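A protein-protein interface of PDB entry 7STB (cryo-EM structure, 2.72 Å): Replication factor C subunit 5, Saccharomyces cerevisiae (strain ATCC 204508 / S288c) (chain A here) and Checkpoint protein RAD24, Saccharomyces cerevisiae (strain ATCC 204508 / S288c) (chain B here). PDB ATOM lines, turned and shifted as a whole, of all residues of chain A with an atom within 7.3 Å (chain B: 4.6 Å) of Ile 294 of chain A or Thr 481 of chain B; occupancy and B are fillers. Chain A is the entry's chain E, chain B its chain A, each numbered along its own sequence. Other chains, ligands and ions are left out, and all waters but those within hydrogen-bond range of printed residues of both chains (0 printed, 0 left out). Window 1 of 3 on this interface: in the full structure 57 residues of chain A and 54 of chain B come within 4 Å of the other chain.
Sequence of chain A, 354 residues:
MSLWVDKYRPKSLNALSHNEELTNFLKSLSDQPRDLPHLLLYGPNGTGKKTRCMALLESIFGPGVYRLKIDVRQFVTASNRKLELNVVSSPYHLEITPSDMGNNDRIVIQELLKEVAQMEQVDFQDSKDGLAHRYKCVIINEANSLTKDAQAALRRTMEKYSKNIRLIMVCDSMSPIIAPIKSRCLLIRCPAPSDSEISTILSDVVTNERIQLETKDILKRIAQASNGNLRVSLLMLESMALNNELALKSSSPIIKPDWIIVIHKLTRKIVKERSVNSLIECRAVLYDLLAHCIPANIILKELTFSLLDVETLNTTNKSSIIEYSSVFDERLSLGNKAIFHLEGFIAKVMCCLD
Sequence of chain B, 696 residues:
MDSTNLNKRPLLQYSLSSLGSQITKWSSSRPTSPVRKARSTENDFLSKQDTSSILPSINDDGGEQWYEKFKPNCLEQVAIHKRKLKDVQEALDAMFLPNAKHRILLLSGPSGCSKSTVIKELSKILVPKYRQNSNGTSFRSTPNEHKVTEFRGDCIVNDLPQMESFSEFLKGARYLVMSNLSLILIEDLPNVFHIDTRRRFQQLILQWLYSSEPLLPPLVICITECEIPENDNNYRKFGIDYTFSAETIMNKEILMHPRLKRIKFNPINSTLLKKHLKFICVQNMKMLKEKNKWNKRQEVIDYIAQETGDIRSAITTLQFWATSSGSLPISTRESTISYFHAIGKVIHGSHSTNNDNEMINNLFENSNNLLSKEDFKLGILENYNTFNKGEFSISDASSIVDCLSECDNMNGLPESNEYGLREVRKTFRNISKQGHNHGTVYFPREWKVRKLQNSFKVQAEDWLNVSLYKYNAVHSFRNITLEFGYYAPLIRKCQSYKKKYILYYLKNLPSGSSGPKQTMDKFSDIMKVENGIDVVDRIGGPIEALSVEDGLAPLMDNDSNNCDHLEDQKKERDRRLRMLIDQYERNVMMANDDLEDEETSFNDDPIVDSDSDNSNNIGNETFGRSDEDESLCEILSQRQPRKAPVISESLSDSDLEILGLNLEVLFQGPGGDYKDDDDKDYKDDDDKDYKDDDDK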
ATOM      1  N   ASP A 258     -18.100 -27.914  22.765  1.00  0.00           N
ATOM      2  CA  ASP A 258     -18.903 -27.873  23.984  1.00  0.00           C
ATOM      3  C   ASP A 258     -19.736 -26.598  24.061  1.00  0.00           C
ATOM      4  O   ASP A 258     -20.912 -26.639  24.443  1.00  0.00           O
ATOM      5  CB  ASP A 258     -18.001 -28.001  25.211  1.00  0.00           C
ATOM      6  CG  ASP A 258     -16.765 -27.128  25.124  1.00  0.00           C
ATOM      7  OD1 ASP A 258     -16.540 -26.519  24.058  1.00  0.00           O
ATOM      8  OD2 ASP A 258     -16.018 -27.052  26.121  1.00  0.00           O
ATOM      9  N   TRP A 259     -19.144 -25.454  23.708  1.00  0.00           N
ATOM     10  CA  TRP A 259     -19.883 -24.198  23.796  1.00  0.00           C
ATOM     11  C   TRP A 259     -21.083 -24.189  22.857  1.00  0.00           C
ATOM     12  O   TRP A 259     -22.096 -23.551  23.157  1.00  0.00           O
ATOM     13  CB  TRP A 259     -18.960 -23.009  23.510  1.00  0.00           C
ATOM     14  CG  TRP A 259     -18.244 -23.053  22.188  1.00  0.00           C
ATOM     15  CD1 TRP A 259     -17.191 -23.850  21.849  1.00  0.00           C
ATOM     16  CD2 TRP A 259     -18.525 -22.249  21.036  1.00  0.00           C
ATOM     17  NE1 TRP A 259     -16.802 -23.598  20.555  1.00  0.00           N
ATOM     18  CE2 TRP A 259     -17.605 -22.618  20.035  1.00  0.00           C
ATOM     19  CE3 TRP A 259     -19.465 -21.255  20.753  1.00  0.00           C
ATOM     20  CZ2 TRP A 259     -17.600 -22.029  18.773  1.00  0.00           C
ATOM     21  CZ3 TRP A 259     -19.459 -20.672  19.501  1.00  0.00           C
ATOM     22  CH2 TRP A 259     -18.532 -21.061  18.526  1.00  0.00           C
ATOM     23  N   ILE A 263     -24.813 -23.434  24.111  1.00  0.00           N
ATOM     24  CA  ILE A 263     -25.663 -22.397  23.530  1.00  0.00           C
ATOM     25  C   ILE A 263     -27.014 -22.976  23.129  1.00  0.00           C
ATOM     26  O   ILE A 263     -28.057 -22.343  23.326  1.00  0.00           O
ATOM     27  CB  ILE A 263     -24.952 -21.728  22.339  1.00  0.00           C
ATOM     28  CG1 ILE A 263     -23.961 -20.678  22.845  1.00  0.00           C
ATOM     29  CG2 ILE A 263     -25.965 -21.091  21.393  1.00  0.00           C
ATOM     30  CD1 ILE A 263     -22.958 -20.224  21.806  1.00  0.00           C
ATOM     31  N   LEU A 286     -24.128 -17.184  30.381  1.00  0.00           N
ATOM     32  CA  LEU A 286     -23.436 -16.167  29.593  1.00  0.00           C
ATOM     33  C   LEU A 286     -22.091 -15.809  30.216  1.00  0.00           C
ATOM     34  O   LEU A 286     -21.084 -15.674  29.507  1.00  0.00           O
ATOM     35  CB  LEU A 286     -24.312 -14.922  29.454  1.00  0.00           C
ATOM     36  CG  LEU A 286     -25.413 -14.986  28.393  1.00  0.00           C
ATOM     37  CD1 LEU A 286     -26.342 -13.791  28.524  1.00  0.00           C
ATOM     38  CD2 LEU A 286     -24.819 -15.051  26.995  1.00  0.00           C
ATOM     39  N   ASP A 288     -20.251 -17.783  32.088  1.00  0.00           N
ATOM     40  CA  ASP A 288     -19.333 -18.900  31.881  1.00  0.00           C
ATOM     41  C   ASP A 288     -18.777 -18.892  30.460  1.00  0.00           C
ATOM     42  O   ASP A 288     -17.565 -19.056  30.251  1.00  0.00           O
ATOM     43  CB  ASP A 288     -20.042 -20.219  32.178  1.00  0.00           C
ATOM     44  CG  ASP A 288     -19.106 -21.408  32.120  1.00  0.00           C
ATOM     45  OD1 ASP A 288     -18.298 -21.575  33.058  1.00  0.00           O
ATOM     46  OD2 ASP A 288     -19.176 -22.172  31.139  1.00  0.00           O
ATOM     47  N   LEU A 289     -19.647 -18.677  29.470  1.00  0.00           N
ATOM     48  CA  LEU A 289     -19.194 -18.635  28.083  1.00  0.00           C
ATOM     49  C   LEU A 289     -18.183 -17.516  27.871  1.00  0.00           C
ATOM     50  O   LEU A 289     -17.167 -17.709  27.193  1.00  0.00           O
ATOM     51  CB  LEU A 289     -20.388 -18.460  27.147  1.00  0.00           C
ATOM     52  CG  LEU A 289     -21.257 -19.699  26.928  1.00  0.00           C
ATOM     53  CD1 LEU A 289     -22.581 -19.315  26.287  1.00  0.00           C
ATOM     54  CD2 LEU A 289     -20.529 -20.727  26.076  1.00  0.00           C
ATOM     55  N   LEU A 290     -18.441 -16.338  28.441  1.00  0.00           N
ATOM     56  CA  LEU A 290     -17.488 -15.239  28.319  1.00  0.00           C
ATOM     57  C   LEU A 290     -16.185 -15.557  29.043  1.00  0.00           C
ATOM     58  O   LEU A 290     -15.101 -15.206  28.565  1.00  0.00           O
ATOM     59  CB  LEU A 290     -18.104 -13.949  28.857  1.00  0.00           C
ATOM     60  CG  LEU A 290     -19.237 -13.354  28.016  1.00  0.00           C
ATOM     61  CD1 LEU A 290     -19.930 -12.231  28.771  1.00  0.00           C
ATOM     62  CD2 LEU A 290     -18.714 -12.856  26.678  1.00  0.00           C
ATOM     63  N   ALA A 291     -16.273 -16.219  30.198  1.00  0.00           N
ATOM     64  CA  ALA A 291     -15.083 -16.608  30.941  1.00  0.00           C
ATOM     65  C   ALA A 291     -14.240 -17.610  30.172  1.00  0.00           C
ATOM     66  O   ALA A 291     -13.030 -17.700  30.411  1.00  0.00           O
ATOM     67  CB  ALA A 291     -15.482 -17.191  32.297  1.00  0.00           C
ATOM     68  N   HIS A 292     -14.847 -18.361  29.255  1.00  0.00           N
ATOM     69  CA  HIS A 292     -14.080 -19.201  28.344  1.00  0.00           C
ATOM     70  C   HIS A 292     -13.489 -18.410  27.172  1.00  0.00           C
ATOM     71  O   HIS A 292     -13.080 -19.012  26.171  1.00  0.00           O
ATOM     72  CB  HIS A 292     -14.951 -20.348  27.825  1.00  0.00           C
ATOM     73  CG  HIS A 292     -14.908 -21.569  28.689  1.00  0.00           C
ATOM     74  ND1 HIS A 292     -15.458 -21.607  29.952  1.00  0.00           N
ATOM     75  CD2 HIS A 292     -14.370 -22.793  28.477  1.00  0.00           C
ATOM     76  CE1 HIS A 292     -15.267 -22.804  30.478  1.00  0.00           C
ATOM     77  NE2 HIS A 292     -14.609 -23.542  29.602  1.00  0.00           N
ATOM     78  N   CYS A 293     -13.439 -17.081  27.281  1.00  0.00           N
ATOM     79  CA  CYS A 293     -12.824 -16.214  26.274  1.00  0.00           C
ATOM     80  C   CYS A 293     -13.517 -16.332  24.920  1.00  0.00           C
ATOM     81  O   CYS A 293     -12.917 -16.058  23.878  1.00  0.00           O
ATOM     82  CB  CYS A 293     -11.328 -16.505  26.132  1.00  0.00           C
ATOM     83  SG  CYS A 293     -10.322 -15.869  27.490  1.00  0.00           S
ATOM     84  N   ILE A 294     -14.780 -16.732  24.918  1.00  0.00           N
ATOM     85  CA  ILE A 294     -15.554 -16.776  23.678  1.00  0.00           C
ATOM     86  C   ILE A 294     -15.976 -15.353  23.318  1.00  0.00           C
ATOM     87  O   ILE A 294     -16.530 -14.649  24.177  1.00  0.00           O
ATOM     88  CB  ILE A 294     -16.768 -17.688  23.828  1.00  0.00           C
ATOM     89  CG1 ILE A 294     -16.360 -19.054  24.396  1.00  0.00           C
ATOM     90  CG2 ILE A 294     -17.470 -17.861  22.487  1.00  0.00           C
ATOM     91  CD1 ILE A 294     -15.482 -19.880  23.475  1.00  0.00           C
ATOM     92  N   PRO A 295     -15.733 -14.889  22.091  1.00  0.00           N
ATOM     93  CA  PRO A 295     -16.100 -13.509  21.747  1.00  0.00           C
ATOM     94  C   PRO A 295     -17.585 -13.251  21.958  1.00  0.00           C
ATOM     95  O   PRO A 295     -18.426 -14.126  21.750  1.00  0.00           O
ATOM     96  CB  PRO A 295     -15.715 -13.397  20.269  1.00  0.00           C
ATOM     97  CG  PRO A 295     -14.661 -14.417  20.073  1.00  0.00           C
ATOM     98  CD  PRO A 295     -14.994 -15.546  20.999  1.00  0.00           C
ATOM     99  N   ALA A 296     -17.902 -12.027  22.388  1.00  0.00           N
ATOM    100  CA  ALA A 296     -19.297 -11.662  22.604  1.00  0.00           C
ATOM    101  C   ALA A 296     -20.088 -11.699  21.302  1.00  0.00           C
ATOM    102  O   ALA A 296     -21.243 -12.141  21.280  1.00  0.00           O
ATOM    103  CB  ALA A 296     -19.382 -10.277  23.243  1.00  0.00           C
ATOM    104  N   ASN A 297     -19.487 -11.229  20.206  1.00  0.00           N
ATOM    105  CA  ASN A 297     -20.204 -11.188  18.934  1.00  0.00           C
ATOM    106  C   ASN A 297     -20.551 -12.589  18.446  1.00  0.00           C
ATOM    107  O   ASN A 297     -21.671 -12.828  17.974  1.00  0.00           O
ATOM    108  CB  ASN A 297     -19.379 -10.447  17.879  1.00  0.00           C
ATOM    109  CG  ASN A 297     -17.916 -10.847  17.890  1.00  0.00           C
ATOM    110  OD1 ASN A 297     -17.189 -10.566  18.842  1.00  0.00           O
ATOM    111  ND2 ASN A 297     -17.476 -11.506  16.824  1.00  0.00           N
ATOM    112  N   ILE A 298     -19.610 -13.530  18.541  1.00  0.00           N
ATOM    113  CA  ILE A 298     -19.895 -14.893  18.101  1.00  0.00           C
ATOM    114  C   ILE A 298     -20.926 -15.538  19.019  1.00  0.00           C
ATOM    115  O   ILE A 298     -21.779 -16.310  18.567  1.00  0.00           O
ATOM    116  CB  ILE A 298     -18.597 -15.721  18.015  1.00  0.00           C
ATOM    117  CG1 ILE A 298     -18.765 -16.892  17.042  1.00  0.00           C
ATOM    118  CG2 ILE A 298     -18.186 -16.256  19.374  1.00  0.00           C
ATOM    119  CD1 ILE A 298     -18.981 -16.477  15.600  1.00  0.00           C
ATOM    120  N   ILE A 299     -20.868 -15.234  20.317  1.00  0.00           N
ATOM    121  CA  ILE A 299     -21.895 -15.719  21.238  1.00  0.00           C
ATOM    122  C   ILE A 299     -23.266 -15.239  20.789  1.00  0.00           C
ATOM    123  O   ILE A 299     -24.224 -16.018  20.707  1.00  0.00           O
ATOM    124  CB  ILE A 299     -21.592 -15.261  22.676  1.00  0.00           C
ATOM    125  CG1 ILE A 299     -20.382 -16.006  23.237  1.00  0.00           C
ATOM    126  CG2 ILE A 299     -22.812 -15.473  23.567  1.00  0.00           C
ATOM    127  CD1 ILE A 299     -19.877 -15.443  24.550  1.00  0.00           C
ATOM    128  N   LEU A 342     -25.968  -8.537  25.485  1.00  0.00           N
ATOM    129  CA  LEU A 342     -26.433  -9.919  25.410  1.00  0.00           C
ATOM    130  C   LEU A 342     -27.648 -10.130  26.306  1.00  0.00           C
ATOM    131  O   LEU A 342     -28.645 -10.743  25.896  1.00  0.00           O
ATOM    132  CB  LEU A 342     -25.302 -10.872  25.800  1.00  0.00           C
ATOM    133  CG  LEU A 342     -24.013 -10.752  24.984  1.00  0.00           C
ATOM    134  CD1 LEU A 342     -22.922 -11.623  25.581  1.00  0.00           C
ATOM    135  CD2 LEU A 342     -24.257 -11.120  23.530  1.00  0.00           C
ATOM    136  N   PHE B 456      -7.403 -18.483  31.152  1.00  0.00           N
ATOM    137  CA  PHE B 456      -7.565 -19.060  29.823  1.00  0.00           C
ATOM    138  C   PHE B 456      -6.481 -18.565  28.876  1.00  0.00           C
ATOM    139  O   PHE B 456      -5.958 -19.336  28.067  1.00  0.00           O
ATOM    140  CB  PHE B 456      -8.951 -18.723  29.275  1.00  0.00           C
ATOM    141  CG  PHE B 456      -9.366 -19.572  28.107  1.00  0.00           C
ATOM    142  CD1 PHE B 456      -8.847 -19.341  26.845  1.00  0.00           C
ATOM    143  CD2 PHE B 456     -10.280 -20.598  28.273  1.00  0.00           C
ATOM    144  CE1 PHE B 456      -9.229 -20.119  25.772  1.00  0.00           C
ATOM    145  CE2 PHE B 456     -10.666 -21.378  27.202  1.00  0.00           C
ATOM    146  CZ  PHE B 456     -10.141 -21.139  25.950  1.00  0.00           C
ATOM    147  N   PHE B 477      -4.860 -17.394  18.472  1.00  0.00           N
ATOM    148  CA  PHE B 477      -5.535 -17.539  19.758  1.00  0.00           C
ATOM    149  C   PHE B 477      -7.044 -17.644  19.587  1.00  0.00           C
ATOM    150  O   PHE B 477      -7.716 -18.314  20.382  1.00  0.00           O
ATOM    151  CB  PHE B 477      -5.188 -16.363  20.666  1.00  0.00           C
ATOM    152  CG  PHE B 477      -6.129 -16.198  21.819  1.00  0.00           C
ATOM    153  CD1 PHE B 477      -6.083 -17.062  22.897  1.00  0.00           C
ATOM    154  CD2 PHE B 477      -7.069 -15.181  21.819  1.00  0.00           C
ATOM    155  CE1 PHE B 477      -6.954 -16.912  23.956  1.00  0.00           C
ATOM    156  CE2 PHE B 477      -7.941 -15.028  22.874  1.00  0.00           C
ATOM    157  CZ  PHE B 477      -7.884 -15.892  23.943  1.00  0.00           C
ATOM    158  N   ARG B 478      -7.595 -16.989  18.564  1.00  0.00           N
ATOM    159  CA  ARG B 478      -9.024 -17.100  18.301  1.00  0.00           C
ATOM    160  C   ARG B 478      -9.415 -18.548  18.037  1.00  0.00           C
ATOM    161  O   ARG B 478     -10.429 -19.033  18.554  1.00  0.00           O
ATOM    162  CB  ARG B 478      -9.399 -16.214  17.113  1.00  0.00           C
ATOM    163  CG  ARG B 478     -10.888 -16.113  16.845  1.00  0.00           C
ATOM    164  CD  ARG B 478     -11.166 -15.222  15.646  1.00  0.00           C
ATOM    165  NE  ARG B 478     -12.589 -15.133  15.343  1.00  0.00           N
ATOM    166  CZ  ARG B 478     -13.432 -14.295  15.932  1.00  0.00           C
ATOM    167  NH1 ARG B 478     -13.031 -13.457  16.875  1.00  0.00           N
ATOM    168  NH2 ARG B 478     -14.710 -14.298  15.567  1.00  0.00           N
ATOM    169  N   ASN B 479      -8.613 -19.258  17.241  1.00  0.00           N
ATOM    170  CA  ASN B 479      -8.879 -20.670  16.994  1.00  0.00           C
ATOM    171  C   ASN B 479      -8.769 -21.479  18.280  1.00  0.00           C
ATOM    172  O   ASN B 479      -9.535 -22.426  18.495  1.00  0.00           O
ATOM    173  CB  ASN B 479      -7.916 -21.203  15.935  1.00  0.00           C
ATOM    174  CG  ASN B 479      -8.151 -20.585  14.572  1.00  0.00           C
ATOM    175  OD1 ASN B 479      -9.218 -20.034  14.303  1.00  0.00           O
ATOM    176  ND2 ASN B 479      -7.151 -20.670  13.703  1.00  0.00           N
ATOM    177  N   ILE B 480      -7.820 -21.123  19.149  1.00  0.00           N
ATOM    178  CA  ILE B 480      -7.697 -21.811  20.430  1.00  0.00           C
ATOM    179  C   ILE B 480      -8.975 -21.653  21.239  1.00  0.00           C
ATOM    180  O   ILE B 480      -9.480 -22.617  21.827  1.00  0.00           O
ATOM    181  CB  ILE B 480      -6.470 -21.293  21.203  1.00  0.00           C
ATOM    182  CG1 ILE B 480      -5.183 -21.629  20.444  1.00  0.00           C
ATOM    183  CG2 ILE B 480      -6.443 -21.886  22.608  1.00  0.00           C
ATOM    184  CD1 ILE B 480      -3.936 -20.997  21.031  1.00  0.00           C
ATOM    185  N   THR B 481      -9.519 -20.436  21.284  1.00  0.00           N
ATOM    186  CA  THR B 481     -10.762 -20.217  22.016  1.00  0.00           C
ATOM    187  C   THR B 481     -11.938 -20.936  21.366  1.00  0.00           C
ATOM    188  O   THR B 481     -12.839 -21.405  22.069  1.00  0.00           O
ATOM    189  CB  THR B 481     -11.070 -18.724  22.117  1.00  0.00           C
ATOM    190  OG1 THR B 481     -11.200 -18.169  20.801  1.00  0.00           O
ATOM    191  CG2 THR B 481      -9.972 -17.998  22.866  1.00  0.00           C
ATOM    192  N   LEU B 482     -11.951 -21.035  20.036  1.00  0.00           N
ATOM    193  CA  LEU B 482     -13.143 -21.523  19.350  1.00  0.00           C
ATOM    194  C   LEU B 482     -13.189 -23.050  19.298  1.00  0.00           C
ATOM    195  O   LEU B 482     -14.126 -23.664  19.817  1.00  0.00           O
ATOM    196  CB  LEU B 482     -13.210 -20.933  17.938  1.00  0.00           C
ATOM    197  CG  LEU B 482     -14.120 -19.711  17.777  1.00  0.00           C
ATOM    198  CD1 LEU B 482     -13.810 -18.655  18.830  1.00  0.00           C
ATOM    199  CD2 LEU B 482     -13.991 -19.124  16.379  1.00  0.00           C
ATOM    200  N   GLU B 483     -12.191 -23.682  18.677  1.00  0.00           N
ATOM    201  CA  GLU B 483     -12.264 -25.115  18.406  1.00  0.00           C
ATOM    202  C   GLU B 483     -11.120 -25.926  18.995  1.00  0.00           C
ATOM    203  O   GLU B 483     -11.357 -27.025  19.501  1.00  0.00           O
ATOM    204  CB  GLU B 483     -12.339 -25.360  16.884  1.00  0.00           C
ATOM    205  CG  GLU B 483     -11.072 -25.044  16.091  1.00  0.00           C
ATOM    206  CD  GLU B 483     -10.950 -23.578  15.737  1.00  0.00           C
ATOM    207  OE1 GLU B 483     -11.683 -22.759  16.328  1.00  0.00           O
ATOM    208  OE2 GLU B 483     -10.120 -23.243  14.867  1.00  0.00           O
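The indole nitrogen (NE1) of Trp 259 of chain A lies within hydrogen-bond range of the backbone carbonyl oxygen (O) of Leu 482 of chain B, 2.8 Å away.
The backbone carbonyl oxygen (O) of Arg 478 of chain B sits at hydrogen-bond distance from the side-chain hydroxyl (OG1) of Thr 481 of chain B (2.5 Å). O of Leu 289 of chain A lies close to N of Ile 294 of chain A. The backbone carbonyl oxygen (O) of Asp 288 of chain A sits at hydrogen-bond distance from a ring nitrogen (ND1) of His 292 of chain A (3.3 Å).
His 292 of chain A touches Phe 456 of chain B. Cys 293 of chain A touches Phe 456 of chain B (SG to CB, 3.6 Å). CG2 of Thr 481 of chain B touches O of Cys 293 of chain A, at 3.7 Å. Thr 481 of chain B touches Ile 294 of chain A. Pro 295 of chain A touches Arg 478 of chain B (CG to NH1, 3.7 Å). CD1 of Leu 482 of chain B touches CD of Pro 295 of chain A (3.97 Å).
Of the printed residues of chain B, Ile 294 of chain A touches Thr 481. Thr 481 of chain B touches just these residues of chain A: Cys 293 (3.7 Å) and Ile 294 (3.4 Å). Of the printed residues of chain B, His 292 of chain A touches Phe 456 (3.5 Å). Of the printed residues of chain B, Trp 259 of chain A touches Leu 482 (2.8 Å). The nearest residue of chain A that does not touch Thr 481 of chain B is His 292 of chain A (4.5 Å). The nearest printed residue of chain B that does not touch Pro 295 of chain A is Thr 481 of chain B (4.6 Å).
Printed residues of chain A that touch a printed residue of chain B: Trp 259, His 292, Cys 293, Ile 294 and Pro 295.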
